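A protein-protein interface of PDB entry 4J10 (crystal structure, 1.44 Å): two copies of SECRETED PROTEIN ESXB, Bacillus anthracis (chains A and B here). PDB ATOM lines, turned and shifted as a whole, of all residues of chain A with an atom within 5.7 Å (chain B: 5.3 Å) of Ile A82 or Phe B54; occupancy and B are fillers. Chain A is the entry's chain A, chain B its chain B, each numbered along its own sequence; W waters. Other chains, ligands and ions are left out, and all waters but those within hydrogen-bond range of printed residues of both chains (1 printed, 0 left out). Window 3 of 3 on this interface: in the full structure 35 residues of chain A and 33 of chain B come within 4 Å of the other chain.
Water W1 bridges OD2 of Asp A78 (3.0 Å) and OE1 of Glu B57 (3.4 Å).
The side-chain carboxylate of Asp A78 lies close to the side-chain carboxylate of Glu B57 (2.8 Å).
Of the 13 printed residues of chain A, 5 touch a printed residue of chain B.
Hydrophobic or aromatic side chains of chain A that line the printed part of chain B: Leu A14, Ile A75, Leu A79 and Ile A82.
Hydrophobic or aromatic side chains of chain B that line the printed part of chain A: Trp B46 and Phe B54.
No position is printed for both chains.
Of the 10 pairs that touch across the chains among the printed residues, none has its exchanged pair printed and touching as well.
The side-chain carboxylate (OD1) of Asp A78 lies within salt-bridge range of the guanidinium group (NH2) of Arg A81 (3.1 Å).
The indole nitrogen (NE1) of Trp B46 sits at hydrogen-bond distance from the side-chain amide oxygen (OE1) of Gln B51 (2.8 Å).
Ile A82 touches just these residues of chain B: Trp B46 (3.8 Å) and Phe B54 (3.5 Å).
Of chain A, only Ile A75, Asp A78, Leu A79 and Ile A82 come within 4 Å of Phe B54.
Of the printed residues of chain B, Leu A79 touches Phe B54.
Printed residues of chain B within 4 Å of Leu A14: Trp B46 (3.8 Å).
Printed residues of chain A within 4 Å of Glu B57: Ile A75 and Asp A78.
Of the printed residues of chain B, Ile A75 touches Phe B54, Glu B57 and Phe B58.
Of the printed residues of chain A, Trp B46 touches Leu A14 and Ile A82.
Lys A85 touches none of the printed residues of chain B.
Ala A83 touches none of the printed residues of chain B.
The nearest residue of chain B that does not touch Ile A82 is Thr B50 (4.1 Å).
Trp B46 touches Leu A14 (CZ3 to CD2, 3.8 Å).
CE1 of Phe B54 touches O of Ile A75, at 3.96 Å.
Glu B57 touches Ile A75.
Ile A75 touches Phe B58.
Asp A78 touches Lys B53.
Asp A78 touches Phe B54 (CB to CE1, 3.6 Å).
Phe B54 touches Leu A79.
CZ3 of Trp B46 touches CD1 of Ile A82, 3.8 Å away.
CD1 of Ile A82 touches CE2 of Phe B54 (3.5 Å).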
ATOM      1  N   LEU A  14     -16.507  25.168  -5.849  1.00  0.00           N
ATOM      2  CA  LEU A  14     -17.738  24.409  -5.982  1.00  0.00           C
ATOM      3  C   LEU A  14     -17.955  23.963  -7.424  1.00  0.00           C
ATOM      4  O   LEU A  14     -18.408  22.846  -7.674  1.00  0.00           O
ATOM      5  CB  LEU A  14     -18.925  25.229  -5.488  1.00  0.00           C
ATOM      6  CG  LEU A  14     -18.885  25.505  -3.985  1.00  0.00           C
ATOM      7  CD1 LEU A  14     -19.968  26.478  -3.576  1.00  0.00           C
ATOM      8  CD2 LEU A  14     -19.061  24.193  -3.236  1.00  0.00           C
ATOM      9  N   ILE A  75     -25.790  15.814  -7.377  1.00  0.00           N
ATOM     10  CA  ILE A  75     -24.756  16.442  -6.572  1.00  0.00           C
ATOM     11  C   ILE A  75     -24.115  17.580  -7.350  1.00  0.00           C
ATOM     12  O   ILE A  75     -23.904  18.669  -6.817  1.00  0.00           O
ATOM     13  CB  ILE A  75     -23.703  15.411  -6.122  1.00  0.00           C
ATOM     14  CG1 ILE A  75     -24.348  14.451  -5.115  1.00  0.00           C
ATOM     15  CG2 ILE A  75     -22.487  16.120  -5.521  1.00  0.00           C
ATOM     16  CD1 ILE A  75     -23.497  13.221  -4.812  1.00  0.00           C
ATOM     17  N   THR A  77     -25.434  19.363  -9.811  1.00  0.00           N
ATOM     18  CA  THR A  77     -26.401  20.454  -9.859  1.00  0.00           C
ATOM     19  C   THR A  77     -26.481  21.217  -8.538  1.00  0.00           C
ATOM     20  O   THR A  77     -26.534  22.456  -8.518  1.00  0.00           O
ATOM     21  CB  THR A  77     -27.790  19.913 -10.224  1.00  0.00           C
ATOM     22  OG1 THR A  77     -27.759  19.419 -11.566  1.00  0.00           O
ATOM     23  CG2 THR A  77     -28.846  21.000 -10.125  1.00  0.00           C
ATOM     24  N   ASP A  78     -26.479  20.487  -7.428  1.00  0.00           N
ATOM     25  CA  ASP A  78     -26.596  21.144  -6.126  1.00  0.00           C
ATOM     26  C   ASP A  78     -25.373  22.013  -5.818  1.00  0.00           C
ATOM     27  O   ASP A  78     -25.511  23.114  -5.271  1.00  0.00           O
ATOM     28  CB  ASP A  78     -26.821  20.116  -5.006  1.00  0.00           C
ATOM     29  CG  ASP A  78     -28.209  19.501  -5.050  1.00  0.00           C
ATOM     30  OD1 ASP A  78     -29.078  20.030  -5.771  1.00  0.00           O
ATOM     31  OD2 ASP A  78     -28.431  18.485  -4.358  1.00  0.00           O
ATOM     32  N   LEU A  79     -24.186  21.522  -6.172  1.00  0.00           N
ATOM     33  CA  LEU A  79     -22.960  22.297  -5.994  1.00  0.00           C
ATOM     34  C   LEU A  79     -22.984  23.560  -6.858  1.00  0.00           C
ATOM     35  O   LEU A  79     -22.617  24.643  -6.404  1.00  0.00           O
ATOM     36  CB  LEU A  79     -21.742  21.435  -6.322  1.00  0.00           C
ATOM     37  CG  LEU A  79     -21.457  20.317  -5.318  1.00  0.00           C
ATOM     38  CD1 LEU A  79     -20.513  19.305  -5.943  1.00  0.00           C
ATOM     39  CD2 LEU A  79     -20.883  20.867  -4.011  1.00  0.00           C
ATOM     40  N   LYS A  80     -23.427  23.425  -8.102  1.00  0.00           N
ATOM     41  CA  LYS A  80     -23.512  24.569  -9.000  1.00  0.00           C
ATOM     42  C   LYS A  80     -24.529  25.606  -8.501  1.00  0.00           C
ATOM     43  O   LYS A  80     -24.302  26.812  -8.602  1.00  0.00           O
ATOM     44  CB  LYS A  80     -23.833  24.088 -10.421  1.00  0.00           C
ATOM     45  CG  LYS A  80     -24.101  25.174 -11.442  1.00  0.00           C
ATOM     46  CD  LYS A  80     -22.901  26.097 -11.642  1.00  0.00           C
ATOM     47  CE  LYS A  80     -23.152  27.025 -12.822  1.00  0.00           C
ATOM     48  NZ  LYS A  80     -22.260  28.218 -12.821  1.00  0.00           N
ATOM     49  N   ARG A  81     -25.641  25.137  -7.947  1.00  0.00           N
ATOM     50  CA  ARG A  81     -26.646  26.041  -7.397  1.00  0.00           C
ATOM     51  C   ARG A  81     -26.085  26.878  -6.247  1.00  0.00           C
ATOM     52  O   ARG A  81     -26.364  28.071  -6.144  1.00  0.00           O
ATOM     53  CB  ARG A  81     -27.875  25.253  -6.941  1.00  0.00           C
ATOM     54  CG  ARG A  81     -28.966  26.093  -6.327  1.00  0.00           C
ATOM     55  CD  ARG A  81     -30.325  25.450  -6.549  1.00  0.00           C
ATOM     56  NE  ARG A  81     -30.352  24.037  -6.173  1.00  0.00           N
ATOM     57  CZ  ARG A  81     -31.361  23.451  -5.535  1.00  0.00           C
ATOM     58  NH1 ARG A  81     -32.434  24.153  -5.194  1.00  0.00           N
ATOM     59  NH2 ARG A  81     -31.297  22.161  -5.232  1.00  0.00           N
ATOM     60  N   ILE A  82     -25.273  26.251  -5.398  1.00  0.00           N
ATOM     61  CA  ILE A  82     -24.648  26.980  -4.302  1.00  0.00           C
ATOM     62  C   ILE A  82     -23.573  27.921  -4.839  1.00  0.00           C
ATOM     63  O   ILE A  82     -23.443  29.053  -4.366  1.00  0.00           O
ATOM     64  CB  ILE A  82     -24.086  26.053  -3.214  1.00  0.00           C
ATOM     65  CG1 ILE A  82     -25.214  25.265  -2.565  1.00  0.00           C
ATOM     66  CG2 ILE A  82     -23.344  26.877  -2.150  1.00  0.00           C
ATOM     67  CD1 ILE A  82     -24.734  24.146  -1.677  1.00  0.00           C
ATOM     68  N   ALA A  83     -22.810  27.471  -5.832  1.00  0.00           N
ATOM     69  CA  ALA A  83     -21.824  28.349  -6.466  1.00  0.00           C
ATOM     70  C   ALA A  83     -22.482  29.617  -7.009  1.00  0.00           C
ATOM     71  O   ALA A  83     -21.997  30.728  -6.781  1.00  0.00           O
ATOM     72  CB  ALA A  83     -21.098  27.608  -7.578  1.00  0.00           C
ATOM     73  N   ASP A  84     -23.609  29.448  -7.700  1.00  0.00           N
ATOM     74  CA  ASP A  84     -24.365  30.574  -8.238  1.00  0.00           C
ATOM     75  C   ASP A  84     -24.848  31.517  -7.138  1.00  0.00           C
ATOM     76  O   ASP A  84     -24.773  32.738  -7.274  1.00  0.00           O
ATOM     77  CB  ASP A  84     -25.549  30.066  -9.080  1.00  0.00           C
ATOM     78  CG  ASP A  84     -25.107  29.456 -10.393  1.00  0.00           C
ATOM     79  OD1 ASP A  84     -23.970  29.747 -10.821  1.00  0.00           O
ATOM     80  OD2 ASP A  84     -25.879  28.691 -10.991  1.00  0.00           O
ATOM     81  N   LYS A  85     -25.346  30.947  -6.046  1.00  0.00           N
ATOM     82  CA  LYS A  85     -25.830  31.751  -4.933  1.00  0.00           C
ATOM     83  C   LYS A  85     -24.687  32.573  -4.340  1.00  0.00           C
ATOM     84  O   LYS A  85     -24.853  33.752  -4.033  1.00  0.00           O
ATOM     85  CB  LYS A  85     -26.459  30.863  -3.865  1.00  0.00           C
ATOM     86  CG  LYS A  85     -27.000  31.623  -2.673  1.00  0.00           C
ATOM     87  CD  LYS A  85     -27.529  30.675  -1.608  1.00  0.00           C
ATOM     88  CE  LYS A  85     -26.395  30.138  -0.749  1.00  0.00           C
ATOM     89  NZ  LYS A  85     -26.658  28.750  -0.268  1.00  0.00           N
ATOM     90  N   PHE A  86     -23.522  31.950  -4.203  1.00  0.00           N
ATOM     91  CA  PHE A  86     -22.348  32.653  -3.703  1.00  0.00           C
ATOM     92  C   PHE A  86     -21.962  33.803  -4.614  1.00  0.00           C
ATOM     93  O   PHE A  86     -21.668  34.900  -4.145  1.00  0.00           O
ATOM     94  CB  PHE A  86     -21.166  31.694  -3.579  1.00  0.00           C
ATOM     95  CG  PHE A  86     -21.203  30.839  -2.350  1.00  0.00           C
ATOM     96  CD1 PHE A  86     -22.331  30.790  -1.547  1.00  0.00           C
ATOM     97  CD2 PHE A  86     -20.104  30.080  -1.998  1.00  0.00           C
ATOM     98  CE1 PHE A  86     -22.357  29.999  -0.409  1.00  0.00           C
ATOM     99  CE2 PHE A  86     -20.120  29.291  -0.860  1.00  0.00           C
ATOM    100  CZ  PHE A  86     -21.251  29.251  -0.067  1.00  0.00           C
ATOM    101  N   ARG A  87     -21.969  33.564  -5.918  1.00  0.00           N
ATOM    102  CA  ARG A  87     -21.583  34.598  -6.867  1.00  0.00           C
ATOM    103  C   ARG A  87     -22.557  35.766  -6.902  1.00  0.00           C
ATOM    104  O   ARG A  87     -22.152  36.911  -7.071  1.00  0.00           O
ATOM    105  CB  ARG A  87     -21.439  34.023  -8.271  1.00  0.00           C
ATOM    106  CG  ARG A  87     -20.891  35.026  -9.277  1.00  0.00           C
ATOM    107  CD  ARG A  87     -20.071  34.319 -10.323  1.00  0.00           C
ATOM    108  NE  ARG A  87     -20.378  32.896 -10.330  1.00  0.00           N
ATOM    109  CZ  ARG A  87     -19.474  31.940 -10.507  1.00  0.00           C
ATOM    110  NH1 ARG A  87     -18.201  32.250 -10.699  1.00  0.00           N
ATOM    111  NH2 ARG A  87     -19.851  30.675 -10.492  1.00  0.00           N
ATOM    112  N   ILE B  39     -15.826  15.390  -1.422  1.00  0.00           N
ATOM    113  CA  ILE B  39     -16.829  15.676  -0.395  1.00  0.00           C
ATOM    114  C   ILE B  39     -16.178  15.927   0.962  1.00  0.00           C
ATOM    115  O   ILE B  39     -16.530  16.885   1.665  1.00  0.00           O
ATOM    116  CB  ILE B  39     -17.867  14.538  -0.300  1.00  0.00           C
ATOM    117  CG1 ILE B  39     -18.601  14.388  -1.634  1.00  0.00           C
ATOM    118  CG2 ILE B  39     -18.852  14.803   0.830  1.00  0.00           C
ATOM    119  CD1 ILE B  39     -19.471  15.574  -1.995  1.00  0.00           C
ATOM    120  N   TRP B  46     -17.991  24.950   5.442  1.00  0.00           N
ATOM    121  CA  TRP B  46     -19.326  25.555   5.455  1.00  0.00           C
ATOM    122  C   TRP B  46     -20.189  24.914   6.544  1.00  0.00           C
ATOM    123  O   TRP B  46     -19.710  24.057   7.285  1.00  0.00           O
ATOM    124  CB  TRP B  46     -20.017  25.486   4.080  1.00  0.00           C
ATOM    125  CG  TRP B  46     -20.154  24.110   3.459  1.00  0.00           C
ATOM    126  CD1 TRP B  46     -19.907  22.898   4.050  1.00  0.00           C
ATOM    127  CD2 TRP B  46     -20.556  23.822   2.116  1.00  0.00           C
ATOM    128  NE1 TRP B  46     -20.136  21.881   3.158  1.00  0.00           N
ATOM    129  CE2 TRP B  46     -20.536  22.421   1.958  1.00  0.00           C
ATOM    130  CE3 TRP B  46     -20.945  24.606   1.025  1.00  0.00           C
ATOM    131  CZ2 TRP B  46     -20.870  21.791   0.761  1.00  0.00           C
ATOM    132  CZ3 TRP B  46     -21.273  23.980  -0.170  1.00  0.00           C
ATOM    133  CH2 TRP B  46     -21.230  22.592  -0.289  1.00  0.00           C
ATOM    134  N   THR B  50     -25.410  21.933   5.667  1.00  0.00           N
ATOM    135  CA  THR B  50     -25.099  21.864   4.242  1.00  0.00           C
ATOM    136  C   THR B  50     -24.250  20.638   3.946  1.00  0.00           C
ATOM    137  O   THR B  50     -24.542  19.862   3.027  1.00  0.00           O
ATOM    138  CB  THR B  50     -24.353  23.125   3.759  1.00  0.00           C
ATOM    139  OG1 THR B  50     -25.115  24.292   4.092  1.00  0.00           O
ATOM    140  CG2 THR B  50     -24.142  23.073   2.252  1.00  0.00           C
ATOM    141  N   GLN B  51     -23.196  20.456   4.735  1.00  0.00           N
ATOM    142  CA  GLN B  51     -22.316  19.311   4.569  1.00  0.00           C
ATOM    143  C   GLN B  51     -23.070  17.987   4.719  1.00  0.00           C
ATOM    144  O   GLN B  51     -22.819  17.033   3.976  1.00  0.00           O
ATOM    145  CB  GLN B  51     -21.142  19.392   5.552  1.00  0.00           C
ATOM    146  CG  GLN B  51     -20.152  18.234   5.450  1.00  0.00           C
ATOM    147  CD  GLN B  51     -19.402  18.192   4.129  1.00  0.00           C
ATOM    148  OE1 GLN B  51     -19.459  19.130   3.333  1.00  0.00           O
ATOM    149  NE2 GLN B  51     -18.696  17.091   3.887  1.00  0.00           N
ATOM    150  N   ALA B  52     -24.009  17.944   5.663  1.00  0.00           N
ATOM    151  CA  ALA B  52     -24.780  16.730   5.915  1.00  0.00           C
ATOM    152  C   ALA B  52     -25.616  16.344   4.703  1.00  0.00           C
ATOM    153  O   ALA B  52     -25.757  15.158   4.391  1.00  0.00           O
ATOM    154  CB  ALA B  52     -25.661  16.889   7.148  1.00  0.00           C
ATOM    155  N   LYS B  53     -26.167  17.341   4.016  1.00  0.00           N
ATOM    156  CA  LYS B  53     -26.955  17.073   2.816  1.00  0.00           C
ATOM    157  C   LYS B  53     -26.103  16.434   1.732  1.00  0.00           C
ATOM    158  O   LYS B  53     -26.496  15.435   1.134  1.00  0.00           O
ATOM    159  CB  LYS B  53     -27.616  18.350   2.287  1.00  0.00           C
ATOM    160  CG  LYS B  53     -28.405  18.147   0.991  1.00  0.00           C
ATOM    161  CD  LYS B  53     -29.135  19.422   0.576  1.00  0.00           C
ATOM    162  CE  LYS B  53     -29.745  19.299  -0.816  1.00  0.00           C
ATOM    163  NZ  LYS B  53     -30.508  20.523  -1.197  1.00  0.00           N
ATOM    164  N   PHE B  54     -24.923  16.992   1.481  1.00  0.00           N
ATOM    165  CA  PHE B  54     -24.039  16.424   0.474  1.00  0.00           C
ATOM    166  C   PHE B  54     -23.494  15.056   0.864  1.00  0.00           C
ATOM    167  O   PHE B  54     -23.362  14.183   0.011  1.00  0.00           O
ATOM    168  CB  PHE B  54     -22.912  17.396   0.127  1.00  0.00           C
ATOM    169  CG  PHE B  54     -23.361  18.528  -0.741  1.00  0.00           C
ATOM    170  CD1 PHE B  54     -23.537  18.335  -2.107  1.00  0.00           C
ATOM    171  CD2 PHE B  54     -23.634  19.771  -0.201  1.00  0.00           C
ATOM    172  CE1 PHE B  54     -23.974  19.372  -2.916  1.00  0.00           C
ATOM    173  CE2 PHE B  54     -24.067  20.812  -1.008  1.00  0.00           C
ATOM    174  CZ  PHE B  54     -24.236  20.602  -2.371  1.00  0.00           C
ATOM    175  N   ARG B  55     -23.197  14.870   2.151  1.00  0.00           N
ATOM    176  CA  ARG B  55     -22.739  13.565   2.628  1.00  0.00           C
ATOM    177  C   ARG B  55     -23.841  12.536   2.418  1.00  0.00           C
ATOM    178  O   ARG B  55     -23.573  11.409   2.013  1.00  0.00           O
ATOM    179  CB  ARG B  55     -22.354  13.626   4.108  1.00  0.00           C
ATOM    180  CG  ARG B  55     -21.814  12.314   4.664  1.00  0.00           C
ATOM    181  CD  ARG B  55     -20.489  11.951   4.030  1.00  0.00           C
ATOM    182  NE  ARG B  55     -19.421  12.845   4.471  1.00  0.00           N
ATOM    183  CZ  ARG B  55     -18.181  12.825   3.989  1.00  0.00           C
ATOM    184  NH1 ARG B  55     -17.850  11.960   3.041  1.00  0.00           N
ATOM    185  NH2 ARG B  55     -17.274  13.678   4.453  1.00  0.00           N
ATOM    186  N   GLY B  56     -25.082  12.940   2.676  1.00  0.00           N
ATOM    187  CA  GLY B  56     -26.219  12.051   2.512  1.00  0.00           C
ATOM    188  C   GLY B  56     -26.395  11.625   1.067  1.00  0.00           C
ATOM    189  O   GLY B  56     -26.571  10.442   0.776  1.00  0.00           O
ATOM    190  N   GLU B  57     -26.346  12.594   0.156  1.00  0.00           N
ATOM    191  CA  GLU B  57     -26.464  12.308  -1.268  1.00  0.00           C
ATOM    192  C   GLU B  57     -25.317  11.421  -1.711  1.00  0.00           C
ATOM    193  O   GLU B  57     -25.502  10.474  -2.478  1.00  0.00           O
ATOM    194  CB  GLU B  57     -26.463  13.609  -2.078  1.00  0.00           C
ATOM    195  CG  GLU B  57     -27.727  14.436  -1.892  1.00  0.00           C
ATOM    196  CD  GLU B  57     -27.665  15.781  -2.591  1.00  0.00           C
ATOM    197  OE1 GLU B  57     -26.882  15.927  -3.549  1.00  0.00           O
ATOM    198  OE2 GLU B  57     -28.411  16.692  -2.184  1.00  0.00           O
ATOM    199  N   PHE B  58     -24.122  11.723  -1.219  1.00  0.00           N
ATOM    200  CA  PHE B  58     -22.970  10.949  -1.613  1.00  0.00           C
ATOM    201  C   PHE B  58     -23.074   9.500  -1.123  1.00  0.00           C
ATOM    202  O   PHE B  58     -22.728   8.563  -1.848  1.00  0.00           O
ATOM    203  CB  PHE B  58     -21.659  11.596  -1.171  1.00  0.00           C
ATOM    204  CG  PHE B  58     -20.468  10.874  -1.707  1.00  0.00           C
ATOM    205  CD1 PHE B  58     -20.196  10.899  -3.069  1.00  0.00           C
ATOM    206  CD2 PHE B  58     -19.673  10.103  -0.883  1.00  0.00           C
ATOM    207  CE1 PHE B  58     -19.125  10.201  -3.595  1.00  0.00           C
ATOM    208  CE2 PHE B  58     -18.597   9.392  -1.409  1.00  0.00           C
ATOM    209  CZ  PHE B  58     -18.326   9.447  -2.761  1.00  0.00           C
ATOM    210  N   ILE B  59     -23.572   9.316   0.094  1.00  0.00           N
ATOM    211  CA  ILE B  59     -23.776   7.969   0.622  1.00  0.00           C
ATOM    212  C   ILE B  59     -24.756   7.166  -0.241  1.00  0.00           C
ATOM    213  O   ILE B  59     -24.560   5.966  -0.453  1.00  0.00           O
ATOM    214  CB  ILE B  59     -24.220   8.009   2.097  1.00  0.00           C
ATOM    215  CG1 ILE B  59     -23.025   8.384   2.974  1.00  0.00           C
ATOM    216  CG2 ILE B  59     -24.801   6.668   2.535  1.00  0.00           C
ATOM    217  CD1 ILE B  59     -23.400   8.831   4.359  1.00  0.00           C
HETATM  218  O   HOH W   1     -29.434  16.023  -5.718  1.00  0.00           O
